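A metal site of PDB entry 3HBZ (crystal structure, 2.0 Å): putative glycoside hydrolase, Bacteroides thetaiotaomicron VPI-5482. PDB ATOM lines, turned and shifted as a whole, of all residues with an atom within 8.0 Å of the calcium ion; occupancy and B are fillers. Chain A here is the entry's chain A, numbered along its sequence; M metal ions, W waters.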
ATOM      1  N   TYR A 100      17.314  36.084   2.248  1.00  0.00           N
ATOM      2  CA  TYR A 100      17.232  34.728   2.800  1.00  0.00           C
ATOM      3  C   TYR A 100      16.419  33.817   1.906  1.00  0.00           C
ATOM      4  O   TYR A 100      15.209  33.948   1.820  1.00  0.00           O
ATOM      5  CB  TYR A 100      16.577  34.774   4.175  1.00  0.00           C
ATOM      6  CG  TYR A 100      17.076  35.907   5.045  1.00  0.00           C
ATOM      7  CD1 TYR A 100      18.417  36.039   5.338  1.00  0.00           C
ATOM      8  CD2 TYR A 100      16.198  36.835   5.565  1.00  0.00           C
ATOM      9  CE1 TYR A 100      18.884  37.063   6.125  1.00  0.00           C
ATOM     10  CE2 TYR A 100      16.644  37.885   6.349  1.00  0.00           C
ATOM     11  CZ  TYR A 100      17.978  37.991   6.654  1.00  0.00           C
ATOM     12  OH  TYR A 100      18.410  39.034   7.461  1.00  0.00           O
ATOM     13  N   ASN A 101      17.083  32.866   1.257  1.00  0.00           N
ATOM     14  CA  ASN A 101      16.406  31.936   0.352  1.00  0.00           C
ATOM     15  C   ASN A 101      16.313  30.500   0.921  1.00  0.00           C
ATOM     16  O   ASN A 101      15.707  29.611   0.324  1.00  0.00           O
ATOM     17  CB  ASN A 101      17.119  31.961  -1.005  1.00  0.00           C
ATOM     18  CG  ASN A 101      16.741  33.190  -1.837  1.00  0.00           C
ATOM     19  OD1 ASN A 101      15.595  33.368  -2.204  1.00  0.00           O
ATOM     20  ND2 ASN A 101      17.710  34.038  -2.133  1.00  0.00           N
ATOM     21  N   PHE A 102      16.937  30.291   2.076  1.00  0.00           N
ATOM     22  CA  PHE A 102      16.861  29.047   2.828  1.00  0.00           C
ATOM     23  C   PHE A 102      17.334  27.827   2.071  1.00  0.00           C
ATOM     24  O   PHE A 102      16.808  26.723   2.292  1.00  0.00           O
ATOM     25  CB  PHE A 102      15.443  28.908   3.419  1.00  0.00           C
ATOM     26  CG  PHE A 102      15.089  30.063   4.327  1.00  0.00           C
ATOM     27  CD1 PHE A 102      15.642  30.144   5.578  1.00  0.00           C
ATOM     28  CD2 PHE A 102      14.345  31.143   3.870  1.00  0.00           C
ATOM     29  CE1 PHE A 102      15.393  31.237   6.391  1.00  0.00           C
ATOM     30  CE2 PHE A 102      14.103  32.228   4.691  1.00  0.00           C
ATOM     31  CZ  PHE A 102      14.640  32.259   5.949  1.00  0.00           C
ATOM     32  N   GLU A 103      18.321  28.017   1.188  1.00  0.00           N
ATOM     33  CA  GLU A 103      18.907  26.952   0.417  1.00  0.00           C
ATOM     34  C   GLU A 103      20.056  26.228   1.151  1.00  0.00           C
ATOM     35  O   GLU A 103      20.293  25.062   0.919  1.00  0.00           O
ATOM     36  CB  GLU A 103      19.444  27.445  -0.940  1.00  0.00           C
ATOM     37  CG  GLU A 103      18.461  28.267  -1.832  1.00  0.00           C
ATOM     38  CD  GLU A 103      17.144  27.545  -2.064  1.00  0.00           C
ATOM     39  OE1 GLU A 103      17.151  26.287  -2.087  1.00  0.00           O
ATOM     40  OE2 GLU A 103      16.109  28.223  -2.211  1.00  0.00           O
ATOM     41  N   ASP A 104      20.783  26.946   1.993  1.00  0.00           N
ATOM     42  CA  ASP A 104      22.089  26.479   2.465  1.00  0.00           C
ATOM     43  C   ASP A 104      22.006  26.055   3.921  1.00  0.00           C
ATOM     44  O   ASP A 104      21.480  26.799   4.769  1.00  0.00           O
ATOM     45  CB  ASP A 104      23.099  27.608   2.390  1.00  0.00           C
ATOM     46  CG  ASP A 104      23.458  27.993   0.940  1.00  0.00           C
ATOM     47  OD1 ASP A 104      23.603  27.101   0.085  1.00  0.00           O
ATOM     48  OD2 ASP A 104      23.552  29.185   0.681  1.00  0.00           O
ATOM     49  N   GLN A 149      14.615  21.692   6.887  1.00  0.00           N
ATOM     50  CA  GLN A 149      14.536  22.213   5.524  1.00  0.00           C
ATOM     51  C   GLN A 149      13.622  21.353   4.683  1.00  0.00           C
ATOM     52  O   GLN A 149      13.710  20.132   4.738  1.00  0.00           O
ATOM     53  CB  GLN A 149      15.919  22.208   4.896  1.00  0.00           C
ATOM     54  CG  GLN A 149      16.016  22.969   3.569  1.00  0.00           C
ATOM     55  CD  GLN A 149      17.394  22.880   2.951  1.00  0.00           C
ATOM     56  OE1 GLN A 149      18.012  21.828   2.997  1.00  0.00           O
ATOM     57  NE2 GLN A 149      17.888  23.990   2.377  1.00  0.00           N
ATOM     58  N   PHE A 150      12.786  21.974   3.858  1.00  0.00           N
ATOM     59  CA  PHE A 150      11.792  21.228   3.070  1.00  0.00           C
ATOM     60  C   PHE A 150      12.073  21.465   1.597  1.00  0.00           C
ATOM     61  O   PHE A 150      12.371  22.613   1.212  1.00  0.00           O
ATOM     62  CB  PHE A 150      10.394  21.759   3.429  1.00  0.00           C
ATOM     63  CG  PHE A 150       9.286  21.166   2.636  1.00  0.00           C
ATOM     64  CD1 PHE A 150       9.093  19.789   2.579  1.00  0.00           C
ATOM     65  CD2 PHE A 150       8.390  21.988   1.968  1.00  0.00           C
ATOM     66  CE1 PHE A 150       8.033  19.229   1.861  1.00  0.00           C
ATOM     67  CE2 PHE A 150       7.309  21.445   1.227  1.00  0.00           C
ATOM     68  CZ  PHE A 150       7.128  20.050   1.187  1.00  0.00           C
ATOM     69  N   ALA A 151      11.966  20.428   0.773  1.00  0.00           N
ATOM     70  CA  ALA A 151      12.411  20.510  -0.622  1.00  0.00           C
ATOM     71  C   ALA A 151      11.561  21.434  -1.485  1.00  0.00           C
ATOM     72  O   ALA A 151      12.098  22.052  -2.416  1.00  0.00           O
ATOM     73  CB  ALA A 151      12.589  19.070  -1.316  1.00  0.00           C
ATOM     74  N   ASN A 152      10.270  21.579  -1.165  1.00  0.00           N
ATOM     75  CA  ASN A 152       9.363  22.306  -2.046  1.00  0.00           C
ATOM     76  C   ASN A 152       9.103  23.732  -1.605  1.00  0.00           C
ATOM     77  O   ASN A 152       8.049  24.031  -1.079  1.00  0.00           O
ATOM     78  CB  ASN A 152       8.016  21.587  -2.191  1.00  0.00           C
ATOM     79  CG  ASN A 152       8.145  20.224  -2.843  1.00  0.00           C
ATOM     80  OD1 ASN A 152       8.943  20.022  -3.756  1.00  0.00           O
ATOM     81  ND2 ASN A 152       7.344  19.272  -2.380  1.00  0.00           N
ATOM     82  N   GLY A 153      10.067  24.603  -1.853  1.00  0.00           N
ATOM     83  CA  GLY A 153       9.968  25.995  -1.465  1.00  0.00           C
ATOM     84  C   GLY A 153       9.291  26.782  -2.575  1.00  0.00           C
ATOM     85  O   GLY A 153       8.905  26.227  -3.576  1.00  0.00           O
ATOM     86  N   LYS A 154       9.243  28.096  -2.426  1.00  0.00           N
ATOM     87  CA  LYS A 154       8.688  28.925  -3.447  1.00  0.00           C
ATOM     88  C   LYS A 154       9.649  28.938  -4.634  1.00  0.00           C
ATOM     89  O   LYS A 154       9.227  28.770  -5.751  1.00  0.00           O
ATOM     90  CB  LYS A 154       8.452  30.343  -2.908  1.00  0.00           C
ATOM     91  CG  LYS A 154       7.839  31.311  -3.932  1.00  0.00           C
ATOM     92  CD  LYS A 154       7.244  32.522  -3.243  1.00  0.00           C
ATOM     93  CE  LYS A 154       6.621  33.480  -4.268  1.00  0.00           C
ATOM     94  NZ  LYS A 154       7.655  34.004  -5.210  1.00  0.00           N
ATOM     95  N   THR A 155      10.940  29.138  -4.373  1.00  0.00           N
ATOM     96  CA  THR A 155      11.994  28.842  -5.364  1.00  0.00           C
ATOM     97  C   THR A 155      13.000  28.039  -4.588  1.00  0.00           C
ATOM     98  O   THR A 155      13.297  28.361  -3.456  1.00  0.00           O
ATOM     99  CB  THR A 155      12.645  30.120  -5.947  1.00  0.00           C
ATOM    100  OG1 THR A 155      12.863  31.080  -4.902  1.00  0.00           O
ATOM    101  CG2 THR A 155      11.747  30.766  -7.076  1.00  0.00           C
ATOM    102  N   GLY A 156      13.532  26.983  -5.173  1.00  0.00           N
ATOM    103  CA  GLY A 156      14.410  26.052  -4.434  1.00  0.00           C
ATOM    104  C   GLY A 156      13.735  25.486  -3.196  1.00  0.00           C
ATOM    105  O   GLY A 156      12.560  25.170  -3.222  1.00  0.00           O
ATOM    106  N   LYS A 157      14.497  25.319  -2.115  1.00  0.00           N
ATOM    107  CA  LYS A 157      13.991  24.734  -0.868  1.00  0.00           C
ATOM    108  C   LYS A 157      13.535  25.850   0.017  1.00  0.00           C
ATOM    109  O   LYS A 157      13.700  27.025  -0.360  1.00  0.00           O
ATOM    110  CB  LYS A 157      15.078  23.915  -0.205  1.00  0.00           C
ATOM    111  CG  LYS A 157      15.652  22.850  -1.208  1.00  0.00           C
ATOM    112  CD  LYS A 157      16.844  22.113  -0.625  1.00  0.00           C
ATOM    113  CE  LYS A 157      17.304  20.965  -1.554  1.00  0.00           C
ATOM    114  NZ  LYS A 157      18.604  20.436  -1.073  1.00  0.00           N
ATOM    115  N   CYS A 158      12.953  25.487   1.160  1.00  0.00           N
ATOM    116  CA  CYS A 158      12.531  26.479   2.142  1.00  0.00           C
ATOM    117  C   CYS A 158      12.650  25.990   3.575  1.00  0.00           C
ATOM    118  O   CYS A 158      13.033  24.852   3.838  1.00  0.00           O
ATOM    119  CB  CYS A 158      11.090  26.907   1.877  1.00  0.00           C
ATOM    120  SG  CYS A 158       9.837  25.612   2.239  1.00  0.00           S
ATOM    121  N   LEU A 159      12.364  26.926   4.489  1.00  0.00           N
ATOM    122  CA  LEU A 159      12.346  26.711   5.895  1.00  0.00           C
ATOM    123  C   LEU A 159      10.998  26.097   6.254  1.00  0.00           C
ATOM    124  O   LEU A 159       9.955  26.557   5.774  1.00  0.00           O
ATOM    125  CB  LEU A 159      12.486  28.068   6.621  1.00  0.00           C
ATOM    126  CG  LEU A 159      12.357  28.076   8.152  1.00  0.00           C
ATOM    127  CD1 LEU A 159      13.474  27.206   8.746  1.00  0.00           C
ATOM    128  CD2 LEU A 159      12.380  29.585   8.647  1.00  0.00           C
ATOM    129  N   TRP A 281       1.445  30.368  -1.186  1.00  0.00           N
ATOM    130  CA  TRP A 281       2.530  31.249  -0.744  1.00  0.00           C
ATOM    131  C   TRP A 281       1.970  32.643  -0.676  1.00  0.00           C
ATOM    132  O   TRP A 281       1.482  33.162  -1.691  1.00  0.00           O
ATOM    133  CB  TRP A 281       3.698  31.229  -1.732  1.00  0.00           C
ATOM    134  CG  TRP A 281       4.525  29.939  -1.662  1.00  0.00           C
ATOM    135  CD1 TRP A 281       4.613  28.960  -2.616  1.00  0.00           C
ATOM    136  CD2 TRP A 281       5.372  29.534  -0.606  1.00  0.00           C
ATOM    137  NE1 TRP A 281       5.462  27.972  -2.217  1.00  0.00           N
ATOM    138  CE2 TRP A 281       5.939  28.294  -0.977  1.00  0.00           C
ATOM    139  CE3 TRP A 281       5.725  30.090   0.626  1.00  0.00           C
ATOM    140  CZ2 TRP A 281       6.832  27.606  -0.168  1.00  0.00           C
ATOM    141  CZ3 TRP A 281       6.611  29.397   1.446  1.00  0.00           C
ATOM    142  CH2 TRP A 281       7.161  28.170   1.044  1.00  0.00           C
ATOM    143  N   ILE A 331       8.463  29.037   5.212  1.00  0.00           N
ATOM    144  CA  ILE A 331       8.933  30.383   4.967  1.00  0.00           C
ATOM    145  C   ILE A 331       9.908  30.352   3.816  1.00  0.00           C
ATOM    146  O   ILE A 331      10.747  29.448   3.747  1.00  0.00           O
ATOM    147  CB  ILE A 331       9.650  30.971   6.214  1.00  0.00           C
ATOM    148  CG1 ILE A 331       8.666  31.226   7.379  1.00  0.00           C
ATOM    149  CG2 ILE A 331      10.452  32.213   5.864  1.00  0.00           C
ATOM    150  CD1 ILE A 331       7.712  32.443   7.172  1.00  0.00           C
ATOM    151  N   ASP A 332       9.777  31.299   2.885  1.00  0.00           N
ATOM    152  CA  ASP A 332      10.750  31.418   1.813  1.00  0.00           C
ATOM    153  C   ASP A 332      10.872  32.846   1.293  1.00  0.00           C
ATOM    154  O   ASP A 332       9.977  33.678   1.493  1.00  0.00           O
ATOM    155  CB  ASP A 332      10.395  30.471   0.664  1.00  0.00           C
ATOM    156  CG  ASP A 332      11.648  29.981  -0.113  1.00  0.00           C
ATOM    157  OD1 ASP A 332      12.771  30.385   0.250  1.00  0.00           O
ATOM    158  OD2 ASP A 332      11.497  29.200  -1.097  1.00  0.00           O
ATOM    159  N   GLU A 333      12.007  33.107   0.628  1.00  0.00           N
ATOM    160  CA  GLU A 333      12.257  34.391  -0.083  1.00  0.00           C
ATOM    161  C   GLU A 333      12.062  35.607   0.832  1.00  0.00           C
ATOM    162  O   GLU A 333      11.288  36.525   0.522  1.00  0.00           O
ATOM    163  CB  GLU A 333      11.353  34.515  -1.316  1.00  0.00           C
ATOM    164  CG  GLU A 333      11.619  33.465  -2.370  1.00  0.00           C
ATOM    165  CD  GLU A 333      10.830  33.672  -3.677  1.00  0.00           C
ATOM    166  OE1 GLU A 333      10.065  34.666  -3.790  1.00  0.00           O
ATOM    167  OE2 GLU A 333      10.974  32.836  -4.607  1.00  0.00           O
ATOM    168  N   VAL A 334      12.781  35.647   1.944  1.00  0.00           N
ATOM    169  CA  VAL A 334      12.580  36.721   2.890  1.00  0.00           C
ATOM    170  C   VAL A 334      13.661  37.752   2.641  1.00  0.00           C
ATOM    171  O   VAL A 334      14.782  37.407   2.276  1.00  0.00           O
ATOM    172  CB  VAL A 334      12.686  36.207   4.383  1.00  0.00           C
ATOM    173  CG1 VAL A 334      12.536  37.335   5.380  1.00  0.00           C
ATOM    174  CG2 VAL A 334      11.629  35.158   4.632  1.00  0.00           C
HETATM  175 CA    CA M   1      14.105  29.044  -1.353  1.00  0.00          CA
HETATM  176  O   HOH W   1      14.291  30.994  -2.700  1.00  0.00           O
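Water W1 bridges the side-chain hydroxyl (OG1) of Thr 155 (2.6 Å) and the side-chain amide oxygen (OD1) of Asn 101 (2.8 Å).
The side-chain amide nitrogen (NE2) of Gln 149 lies within hydrogen-bond range of the backbone carbonyl oxygen (O) of Glu 103, at 3.0 Å.
The side-chain hydroxyl (OG1) of Thr 155 is in hydrogen-bond range of the side-chain carboxylate (OE2) of Glu 333, 2.6 Å away.
The side-chain carboxylate (OD2) of Asp 332 lies close to the backbone NH (N) of Lys 154 (2.8 Å).
Five residues have an atom within 4 Å of the calcium ion: Asn 101, Glu 103, Thr 155, Lys 157 and Asp 332.
The nearest printed residue that does not touch the calcium ion is Gly 156 (4.02 Å).
O of Lys 157 binds the calcium ion (2.3 Å).
The calcium ion is bound by the side-chain carboxylate (OE2) of Glu 103 (2.3 Å).
The calcium ion is bound by the backbone carbonyl oxygen (O) of Thr 155, 2.4 Å away.
Water W1 is bound to the calcium ion.
O of Asn 101 is bound to the calcium ion.
OD1 of Asp 332 is bound to the calcium ion (2.5 Å).
OD2 of Asp 332 is bound to the calcium ion (2.6 Å).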
